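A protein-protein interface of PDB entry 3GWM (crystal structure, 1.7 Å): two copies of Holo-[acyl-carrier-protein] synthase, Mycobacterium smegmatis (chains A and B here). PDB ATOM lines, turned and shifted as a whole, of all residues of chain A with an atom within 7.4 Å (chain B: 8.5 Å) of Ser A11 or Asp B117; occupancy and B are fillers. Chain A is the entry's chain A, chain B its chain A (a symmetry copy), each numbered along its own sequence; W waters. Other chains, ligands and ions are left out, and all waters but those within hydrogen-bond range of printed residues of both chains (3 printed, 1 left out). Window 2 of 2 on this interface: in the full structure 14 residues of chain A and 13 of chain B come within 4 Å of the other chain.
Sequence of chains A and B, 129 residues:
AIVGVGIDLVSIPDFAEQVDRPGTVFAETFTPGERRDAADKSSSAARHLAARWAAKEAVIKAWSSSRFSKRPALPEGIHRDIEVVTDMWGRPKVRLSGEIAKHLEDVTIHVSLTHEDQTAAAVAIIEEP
The backbone NH (N) of Leu A9 is in hydrogen-bond range of the side-chain hydroxyl (OG1) of Thr B114. OD1 of Asp B117 is in hydrogen-bond range of OG of Ser A11, 2.6 Å away. The side-chain carboxylate (OD2) of Asp A14 lies close to the side-chain carboxylate (OD2) of Asp B117. The side-chain hydroxyl (OG1) of Thr B114 sits at hydrogen-bond distance from the side-chain carboxylate (OD1) of Asp A8, at 3.4 Å. The backbone NH of Ser A11 lies close to the side-chain carboxylate of Glu B116, at 3.3 Å.
OG of Ser A11 lies within hydrogen-bond range of N of Asp A14 (3.2 Å). The backbone carbonyl oxygen (O) of Ala A120 lies within hydrogen-bond range of the backbone NH (N) of Val A10, 2.9 Å away.
CG of Glu B116 touches O of Leu A9, at 3.4 Å. Leu A9 touches Thr B119. CG of Glu B116 touches N of Val A10, 3.8 Å away. Glu B116 touches Thr A119 (OE2 to CG2, 3.7 Å).
Ser A11 touches just these residues of chain B: Glu B116 and Asp B117. Asp B117 touches two residues of chain A. Printed residues of chain A within 4 Å of Thr B119: Leu A9. Printed residues of chain B within 4 Å of Val A10: Glu B116. Of the printed residues of chain B, Asp A14 touches Asp B117 (2.5 Å). Printed residues of chain B within 4 Å of Leu A9: Thr B114, Glu B116 and Thr B119. Of the printed residues of chain B, Thr A119 touches Glu B116 (3.7 Å). Ser B11 touches none of the printed residues of chain A.
Hydrophobic or aromatic side chains of chain A within 4 Å of the printed part of chain B: Leu A9. Printed residues of chain B that touch a printed residue of chain A: Thr B114, Glu B116, Asp B117 and Thr B119.
Positions printed for both chains: 10, 11, 12, 13, 46, 50, 118, 119 and 120.
Water W3 lies within hydrogen-bond range of OD1 of Asp A14 (2.6 Å) and OD2 of Asp B117 (3.2 Å). Water W2 lies within hydrogen-bond range of the side-chain carboxylate (OD1) of Asp B117 (3.0 Å), the backbone carbonyl oxygen (O) of Gln A118 (3.1 Å) and the side-chain hydroxyl (OG) of Ser A11 (3.3 Å). Water W1 lies within hydrogen-bond range of the side-chain hydroxyl (OG1) of Thr A119 (3.2 Å) and the side-chain hydroxyl (OG1) of Thr B119 (3.2 Å).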
ATOM      1  N   ASP A   8       8.948  -2.876 -35.632  1.00  0.00           N
ATOM      2  CA  ASP A   8       8.855  -2.552 -34.215  1.00  0.00           C
ATOM      3  C   ASP A   8       8.010  -3.589 -33.496  1.00  0.00           C
ATOM      4  O   ASP A   8       6.943  -3.999 -33.990  1.00  0.00           O
ATOM      5  CB  ASP A   8       8.260  -1.158 -33.991  1.00  0.00           C
ATOM      6  CG  ASP A   8       8.554  -0.623 -32.594  1.00  0.00           C
ATOM      7  OD1 ASP A   8       9.746  -0.553 -32.245  1.00  0.00           O
ATOM      8  OD2 ASP A   8       7.611  -0.296 -31.838  1.00  0.00           O
ATOM      9  N   LEU A   9       8.506  -3.991 -32.330  1.00  0.00           N
ATOM     10  CA  LEU A   9       7.841  -4.922 -31.441  1.00  0.00           C
ATOM     11  C   LEU A   9       7.514  -4.157 -30.153  1.00  0.00           C
ATOM     12  O   LEU A   9       8.349  -3.420 -29.634  1.00  0.00           O
ATOM     13  CB  LEU A   9       8.802  -6.063 -31.135  1.00  0.00           C
ATOM     14  CG  LEU A   9       8.313  -7.497 -31.076  1.00  0.00           C
ATOM     15  CD1 LEU A   9       7.296  -7.797 -32.131  1.00  0.00           C
ATOM     16  CD2 LEU A   9       9.532  -8.403 -31.210  1.00  0.00           C
ATOM     17  N   VAL A  10       6.299  -4.326 -29.650  1.00  0.00           N
ATOM     18  CA  VAL A  10       5.845  -3.598 -28.469  1.00  0.00           C
ATOM     19  C   VAL A  10       5.283  -4.589 -27.454  1.00  0.00           C
ATOM     20  O   VAL A  10       4.469  -5.440 -27.795  1.00  0.00           O
ATOM     21  CB  VAL A  10       4.748  -2.559 -28.863  1.00  0.00           C
ATOM     22  CG1 VAL A  10       4.037  -2.003 -27.616  1.00  0.00           C
ATOM     23  CG2 VAL A  10       5.367  -1.429 -29.710  1.00  0.00           C
ATOM     24  N   SER A  11       5.733  -4.484 -26.208  1.00  0.00           N
ATOM     25  CA  SER A  11       5.130  -5.254 -25.115  1.00  0.00           C
ATOM     26  C   SER A  11       3.825  -4.594 -24.709  1.00  0.00           C
ATOM     27  O   SER A  11       3.827  -3.448 -24.292  1.00  0.00           O
ATOM     28  CB  SER A  11       6.063  -5.270 -23.908  1.00  0.00           C
ATOM     29  OG  SER A  11       5.373  -5.744 -22.762  1.00  0.00           O
ATOM     30  N   ILE A  12       2.707  -5.304 -24.818  1.00  0.00           N
ATOM     31  CA  ILE A  12       1.417  -4.693 -24.514  1.00  0.00           C
ATOM     32  C   ILE A  12       1.315  -4.327 -23.024  1.00  0.00           C
ATOM     33  O   ILE A  12       0.847  -3.244 -22.692  1.00  0.00           O
ATOM     34  CB  ILE A  12       0.234  -5.564 -25.013  1.00  0.00           C
ATOM     35  CG1 ILE A  12       0.308  -5.671 -26.544  1.00  0.00           C
ATOM     36  CG2 ILE A  12      -1.105  -4.945 -24.614  1.00  0.00           C
ATOM     37  CD1 ILE A  12      -0.756  -6.542 -27.161  1.00  0.00           C
ATOM     38  N   PRO A  13       1.797  -5.205 -22.133  1.00  0.00           N
ATOM     39  CA  PRO A  13       1.823  -4.832 -20.706  1.00  0.00           C
ATOM     40  C   PRO A  13       2.719  -3.619 -20.400  1.00  0.00           C
ATOM     41  O   PRO A  13       2.349  -2.750 -19.603  1.00  0.00           O
ATOM     42  CB  PRO A  13       2.387  -6.083 -20.023  1.00  0.00           C
ATOM     43  CG  PRO A  13       2.133  -7.208 -20.964  1.00  0.00           C
ATOM     44  CD  PRO A  13       2.159  -6.616 -22.350  1.00  0.00           C
ATOM     45  N   ASP A  14       3.898  -3.559 -21.005  1.00  0.00           N
ATOM     46  CA  ASP A  14       4.783  -2.418 -20.777  1.00  0.00           C
ATOM     47  C   ASP A  14       4.146  -1.140 -21.317  1.00  0.00           C
ATOM     48  O   ASP A  14       4.230  -0.069 -20.700  1.00  0.00           O
ATOM     49  CB  ASP A  14       6.139  -2.646 -21.442  1.00  0.00           C
ATOM     50  CG  ASP A  14       6.947  -3.744 -20.768  1.00  0.00           C
ATOM     51  OD1 ASP A  14       6.464  -4.336 -19.780  1.00  0.00           O
ATOM     52  OD2 ASP A  14       8.075  -4.010 -21.231  1.00  0.00           O
ATOM     53  N   PHE A  15       3.527  -1.253 -22.487  1.00  0.00           N
ATOM     54  CA  PHE A  15       2.870  -0.120 -23.124  1.00  0.00           C
ATOM     55  C   PHE A  15       1.765   0.413 -22.209  1.00  0.00           C
ATOM     56  O   PHE A  15       1.641   1.621 -21.985  1.00  0.00           O
ATOM     57  CB  PHE A  15       2.297  -0.563 -24.480  1.00  0.00           C
ATOM     58  CG  PHE A  15       1.454   0.473 -25.163  1.00  0.00           C
ATOM     59  CD1 PHE A  15       2.045   1.504 -25.890  1.00  0.00           C
ATOM     60  CD2 PHE A  15       0.072   0.411 -25.097  1.00  0.00           C
ATOM     61  CE1 PHE A  15       1.269   2.462 -26.537  1.00  0.00           C
ATOM     62  CE2 PHE A  15      -0.717   1.365 -25.745  1.00  0.00           C
ATOM     63  CZ  PHE A  15      -0.113   2.394 -26.471  1.00  0.00           C
ATOM     64  N   ALA A  16       0.973  -0.497 -21.661  1.00  0.00           N
ATOM     65  CA  ALA A  16      -0.164  -0.100 -20.841  1.00  0.00           C
ATOM     66  C   ALA A  16       0.326   0.672 -19.612  1.00  0.00           C
ATOM     67  O   ALA A  16      -0.337   1.595 -19.133  1.00  0.00           O
ATOM     68  CB  ALA A  16      -0.973  -1.334 -20.424  1.00  0.00           C
ATOM     69  N   GLU A  17       1.494   0.296 -19.113  1.00  0.00           N
ATOM     70  CA  GLU A  17       2.057   0.945 -17.933  1.00  0.00           C
ATOM     71  C   GLU A  17       2.612   2.339 -18.253  1.00  0.00           C
ATOM     72  O   GLU A  17       2.697   3.195 -17.374  1.00  0.00           O
ATOM     73  CB  GLU A  17       3.153   0.065 -17.312  1.00  0.00           C
ATOM     74  CG  GLU A  17       3.520   0.446 -15.889  1.00  0.00           C
ATOM     75  CD  GLU A  17       2.291   0.653 -15.017  1.00  0.00           C
ATOM     76  OE1 GLU A  17       1.449  -0.268 -14.938  1.00  0.00           O
ATOM     77  OE2 GLU A  17       2.161   1.743 -14.418  1.00  0.00           O
ATOM     78  N   ALA A  46      -5.907  -1.520 -24.903  1.00  0.00           N
ATOM     79  CA  ALA A  46      -4.462  -1.674 -24.754  1.00  0.00           C
ATOM     80  C   ALA A  46      -3.871  -2.385 -25.973  1.00  0.00           C
ATOM     81  O   ALA A  46      -2.850  -1.956 -26.515  1.00  0.00           O
ATOM     82  CB  ALA A  46      -4.135  -2.450 -23.483  1.00  0.00           C
ATOM     83  N   ALA A  50      -1.604  -0.399 -28.687  1.00  0.00           N
ATOM     84  CA  ALA A  50      -0.219  -0.866 -28.741  1.00  0.00           C
ATOM     85  C   ALA A  50       0.197  -1.149 -30.196  1.00  0.00           C
ATOM     86  O   ALA A  50       1.323  -0.869 -30.580  1.00  0.00           O
ATOM     87  CB  ALA A  50      -0.036  -2.109 -27.881  1.00  0.00           C
ATOM     88  N   GLN A 118       0.525 -10.910 -25.614  1.00  0.00           N
ATOM     89  CA  GLN A 118       1.141  -9.765 -24.946  1.00  0.00           C
ATOM     90  C   GLN A 118       2.018  -8.933 -25.871  1.00  0.00           C
ATOM     91  O   GLN A 118       2.768  -8.070 -25.406  1.00  0.00           O
ATOM     92  CB  GLN A 118       2.015 -10.249 -23.782  1.00  0.00           C
ATOM     93  CG  GLN A 118       1.473 -11.464 -23.068  1.00  0.00           C
ATOM     94  CD  GLN A 118       0.116 -11.209 -22.480  1.00  0.00           C
ATOM     95  OE1 GLN A 118      -0.092 -10.207 -21.794  1.00  0.00           O
ATOM     96  NE2 GLN A 118      -0.826 -12.113 -22.739  1.00  0.00           N
ATOM     97  N   THR A 119       1.933  -9.180 -27.173  1.00  0.00           N
ATOM     98  CA  THR A 119       2.872  -8.565 -28.112  1.00  0.00           C
ATOM     99  C   THR A 119       2.152  -7.924 -29.302  1.00  0.00           C
ATOM    100  O   THR A 119       1.239  -8.511 -29.875  1.00  0.00           O
ATOM    101  CB  THR A 119       3.875  -9.620 -28.644  1.00  0.00           C
ATOM    102  OG1 THR A 119       4.561 -10.236 -27.539  1.00  0.00           O
ATOM    103  CG2 THR A 119       4.895  -8.977 -29.566  1.00  0.00           C
ATOM    104  N   ALA A 120       2.558  -6.708 -29.657  1.00  0.00           N
ATOM    105  CA  ALA A 120       2.109  -6.095 -30.908  1.00  0.00           C
ATOM    106  C   ALA A 120       3.323  -5.865 -31.795  1.00  0.00           C
ATOM    107  O   ALA A 120       4.451  -5.778 -31.304  1.00  0.00           O
ATOM    108  CB  ALA A 120       1.383  -4.769 -30.641  1.00  0.00           C
ATOM    109  N   VAL B  10      13.695 -13.995 -32.249  1.00  0.00           N
ATOM    110  CA  VAL B  10      14.677 -14.623 -31.370  1.00  0.00           C
ATOM    111  C   VAL B  10      14.185 -14.539 -29.928  1.00  0.00           C
ATOM    112  O   VAL B  10      13.784 -13.477 -29.464  1.00  0.00           O
ATOM    113  CB  VAL B  10      16.058 -13.906 -31.504  1.00  0.00           C
ATOM    114  CG1 VAL B  10      17.018 -14.336 -30.380  1.00  0.00           C
ATOM    115  CG2 VAL B  10      16.664 -14.179 -32.897  1.00  0.00           C
ATOM    116  N   SER B  11      14.206 -15.668 -29.226  1.00  0.00           N
ATOM    117  CA  SER B  11      13.936 -15.671 -27.784  1.00  0.00           C
ATOM    118  C   SER B  11      15.171 -15.182 -27.051  1.00  0.00           C
ATOM    119  O   SER B  11      16.222 -15.795 -27.152  1.00  0.00           O
ATOM    120  CB  SER B  11      13.619 -17.087 -27.313  1.00  0.00           C
ATOM    121  OG  SER B  11      13.655 -17.152 -25.896  1.00  0.00           O
ATOM    122  N   ILE B  12      15.062 -14.089 -26.305  1.00  0.00           N
ATOM    123  CA  ILE B  12      16.237 -13.533 -25.640  1.00  0.00           C
ATOM    124  C   ILE B  12      16.771 -14.495 -24.566  1.00  0.00           C
ATOM    125  O   ILE B  12      17.977 -14.695 -24.472  1.00  0.00           O
ATOM    126  CB  ILE B  12      15.973 -12.101 -25.105  1.00  0.00           C
ATOM    127  CG1 ILE B  12      15.674 -11.174 -26.292  1.00  0.00           C
ATOM    128  CG2 ILE B  12      17.189 -11.571 -24.344  1.00  0.00           C
ATOM    129  CD1 ILE B  12      15.343  -9.755 -25.909  1.00  0.00           C
ATOM    130  N   PRO B  13      15.876 -15.123 -23.792  1.00  0.00           N
ATOM    131  CA  PRO B  13      16.349 -16.140 -22.833  1.00  0.00           C
ATOM    132  C   PRO B  13      17.025 -17.351 -23.501  1.00  0.00           C
ATOM    133  O   PRO B  13      18.049 -17.844 -23.016  1.00  0.00           O
ATOM    134  CB  PRO B  13      15.065 -16.584 -22.124  1.00  0.00           C
ATOM    135  CG  PRO B  13      14.093 -15.472 -22.310  1.00  0.00           C
ATOM    136  CD  PRO B  13      14.445 -14.815 -23.621  1.00  0.00           C
ATOM    137  N   LYS B  41      20.586 -13.392 -19.178  1.00  0.00           N
ATOM    138  CA  LYS B  41      19.381 -13.101 -19.948  1.00  0.00           C
ATOM    139  C   LYS B  41      18.700 -11.795 -19.547  1.00  0.00           C
ATOM    140  O   LYS B  41      17.913 -11.246 -20.314  1.00  0.00           O
ATOM    141  CB  LYS B  41      18.382 -14.251 -19.816  1.00  0.00           C
ATOM    142  CG  LYS B  41      17.775 -14.390 -18.432  1.00  0.00           C
ATOM    143  CD  LYS B  41      16.972 -15.678 -18.315  1.00  0.00           C
ATOM    144  CE  LYS B  41      16.517 -15.925 -16.886  1.00  0.00           C
ATOM    145  NZ  LYS B  41      15.762 -14.760 -16.342  1.00  0.00           N
ATOM    146  N   SER B  42      19.002 -11.300 -18.351  1.00  0.00           N
ATOM    147  CA  SER B  42      18.391 -10.072 -17.854  1.00  0.00           C
ATOM    148  C   SER B  42      19.174  -8.825 -18.265  1.00  0.00           C
ATOM    149  O   SER B  42      18.755  -7.699 -17.980  1.00  0.00           O
ATOM    150  CB  SER B  42      18.296 -10.120 -16.324  1.00  0.00           C
ATOM    151  OG  SER B  42      19.577  -9.959 -15.722  1.00  0.00           O
ATOM    152  N   SER B  43      20.299  -9.023 -18.942  1.00  0.00           N
ATOM    153  CA  SER B  43      21.230  -7.932 -19.199  1.00  0.00           C
ATOM    154  C   SER B  43      20.917  -7.196 -20.499  1.00  0.00           C
ATOM    155  O   SER B  43      20.305  -7.751 -21.420  1.00  0.00           O
ATOM    156  CB  SER B  43      22.666  -8.455 -19.238  1.00  0.00           C
ATOM    157  OG  SER B  43      22.918  -9.166 -20.449  1.00  0.00           O
ATOM    158  N   ALA B  46      22.410  -8.978 -23.401  1.00  0.00           N
ATOM    159  CA  ALA B  46      21.614 -10.068 -23.961  1.00  0.00           C
ATOM    160  C   ALA B  46      20.578  -9.521 -24.946  1.00  0.00           C
ATOM    161  O   ALA B  46      20.415 -10.056 -26.044  1.00  0.00           O
ATOM    162  CB  ALA B  46      20.923 -10.851 -22.852  1.00  0.00           C
ATOM    163  N   ARG B  47      19.880  -8.458 -24.555  1.00  0.00           N
ATOM    164  CA  ARG B  47      18.817  -7.894 -25.394  1.00  0.00           C
ATOM    165  C   ARG B  47      19.356  -7.338 -26.713  1.00  0.00           C
ATOM    166  O   ARG B  47      18.800  -7.597 -27.788  1.00  0.00           O
ATOM    167  CB  ARG B  47      18.061  -6.787 -24.641  1.00  0.00           C
ATOM    168  CG  ARG B  47      17.310  -7.265 -23.394  1.00  0.00           C
ATOM    169  CD  ARG B  47      16.469  -6.143 -22.764  1.00  0.00           C
ATOM    170  NE  ARG B  47      17.286  -5.066 -22.209  1.00  0.00           N
ATOM    171  CZ  ARG B  47      17.682  -4.996 -20.939  1.00  0.00           C
ATOM    172  NH1 ARG B  47      17.341  -5.944 -20.075  1.00  0.00           N
ATOM    173  NH2 ARG B  47      18.432  -3.978 -20.534  1.00  0.00           N
ATOM    174  N   ALA B  50      20.951 -10.093 -28.944  1.00  0.00           N
ATOM    175  CA  ALA B  50      19.886 -10.915 -29.516  1.00  0.00           C
ATOM    176  C   ALA B  50      19.281 -10.228 -30.753  1.00  0.00           C
ATOM    177  O   ALA B  50      18.955 -10.891 -31.728  1.00  0.00           O
ATOM    178  CB  ALA B  50      18.808 -11.196 -28.479  1.00  0.00           C
ATOM    179  N   THR B 114      14.580  -4.820 -33.688  1.00  0.00           N
ATOM    180  CA  THR B 114      13.761  -4.322 -32.601  1.00  0.00           C
ATOM    181  C   THR B 114      13.786  -5.336 -31.476  1.00  0.00           C
ATOM    182  O   THR B 114      14.117  -6.496 -31.693  1.00  0.00           O
ATOM    183  CB  THR B 114      12.303  -4.091 -33.098  1.00  0.00           C
ATOM    184  OG1 THR B 114      11.518  -3.466 -32.075  1.00  0.00           O
ATOM    185  CG2 THR B 114      11.637  -5.410 -33.525  1.00  0.00           C
ATOM    186  N   HIS B 115      13.443  -4.909 -30.264  1.00  0.00           N
ATOM    187  CA  HIS B 115      13.302  -5.865 -29.181  1.00  0.00           C
ATOM    188  C   HIS B 115      12.416  -5.328 -28.075  1.00  0.00           C
ATOM    189  O   HIS B 115      12.274  -4.118 -27.916  1.00  0.00           O
ATOM    190  CB  HIS B 115      14.679  -6.244 -28.617  1.00  0.00           C
ATOM    191  CG  HIS B 115      15.336  -5.147 -27.839  1.00  0.00           C
ATOM    192  ND1 HIS B 115      16.156  -4.206 -28.423  1.00  0.00           N
ATOM    193  CD2 HIS B 115      15.293  -4.842 -26.519  1.00  0.00           C
ATOM    194  CE1 HIS B 115      16.590  -3.368 -27.498  1.00  0.00           C
ATOM    195  NE2 HIS B 115      16.085  -3.735 -26.334  1.00  0.00           N
ATOM    196  N   GLU B 116      11.805  -6.240 -27.332  1.00  0.00           N
ATOM    197  CA  GLU B 116      11.078  -5.876 -26.119  1.00  0.00           C
ATOM    198  C   GLU B 116      10.841  -7.102 -25.274  1.00  0.00           C
ATOM    199  O   GLU B 116      10.527  -8.187 -25.794  1.00  0.00           O
ATOM    200  CB  GLU B 116       9.732  -5.226 -26.430  1.00  0.00           C
ATOM    201  CG  GLU B 116       8.873  -5.970 -27.428  1.00  0.00           C
ATOM    202  CD  GLU B 116       8.116  -7.153 -26.846  1.00  0.00           C
ATOM    203  OE1 GLU B 116       7.711  -7.113 -25.660  1.00  0.00           O
ATOM    204  OE2 GLU B 116       7.898  -8.131 -27.589  1.00  0.00           O
ATOM    205  N   ASP B 117      10.972  -6.911 -23.964  1.00  0.00           N
ATOM    206  CA  ASP B 117      10.754  -7.984 -23.021  1.00  0.00           C
ATOM    207  C   ASP B 117      11.660  -9.140 -23.405  1.00  0.00           C
ATOM    208  O   ASP B 117      12.868  -8.972 -23.403  1.00  0.00           O
ATOM    209  CB  ASP B 117       9.274  -8.370 -22.974  1.00  0.00           C
ATOM    210  CG  ASP B 117       8.436  -7.320 -22.263  1.00  0.00           C
ATOM    211  OD1 ASP B 117       7.210  -7.522 -22.097  1.00  0.00           O
ATOM    212  OD2 ASP B 117       9.021  -6.286 -21.862  1.00  0.00           O
ATOM    213  N   GLN B 118      11.087 -10.291 -23.736  1.00  0.00           N
ATOM    214  CA  GLN B 118      11.876 -11.503 -23.954  1.00  0.00           C
ATOM    215  C   GLN B 118      12.089 -11.820 -25.427  1.00  0.00           C
ATOM    216  O   GLN B 118      12.545 -12.916 -25.767  1.00  0.00           O
ATOM    217  CB  GLN B 118      11.171 -12.705 -23.314  1.00  0.00           C
ATOM    218  CG  GLN B 118      10.441 -12.381 -22.032  1.00  0.00           C
ATOM    219  CD  GLN B 118      11.367 -11.842 -20.980  1.00  0.00           C
ATOM    220  OE1 GLN B 118      12.418 -12.426 -20.714  1.00  0.00           O
ATOM    221  NE2 GLN B 118      10.988 -10.724 -20.369  1.00  0.00           N
ATOM    222  N   THR B 119      11.768 -10.878 -26.306  1.00  0.00           N
ATOM    223  CA  THR B 119      11.761 -11.164 -27.740  1.00  0.00           C
ATOM    224  C   THR B 119      12.527 -10.105 -28.538  1.00  0.00           C
ATOM    225  O   THR B 119      12.379  -8.910 -28.302  1.00  0.00           O
ATOM    226  CB  THR B 119      10.307 -11.235 -28.272  1.00  0.00           C
ATOM    227  OG1 THR B 119       9.569 -12.224 -27.532  1.00  0.00           O
ATOM    228  CG2 THR B 119      10.289 -11.599 -29.745  1.00  0.00           C
ATOM    229  N   ALA B 120      13.363 -10.554 -29.471  1.00  0.00           N
ATOM    230  CA  ALA B 120      13.972  -9.644 -30.443  1.00  0.00           C
ATOM    231  C   ALA B 120      13.505 -10.044 -31.834  1.00  0.00           C
ATOM    232  O   ALA B 120      13.106 -11.190 -32.058  1.00  0.00           O
ATOM    233  CB  ALA B 120      15.504  -9.693 -30.358  1.00  0.00           C
HETATM  234  O   HOH W   1       6.609 -12.383 -28.603  1.00  0.00           O
HETATM  235  O   HOH W   2       5.214  -8.916 -23.770  1.00  0.00           O
HETATM  236  O   HOH W   3       7.900  -6.229 -18.843  1.00  0.00           O
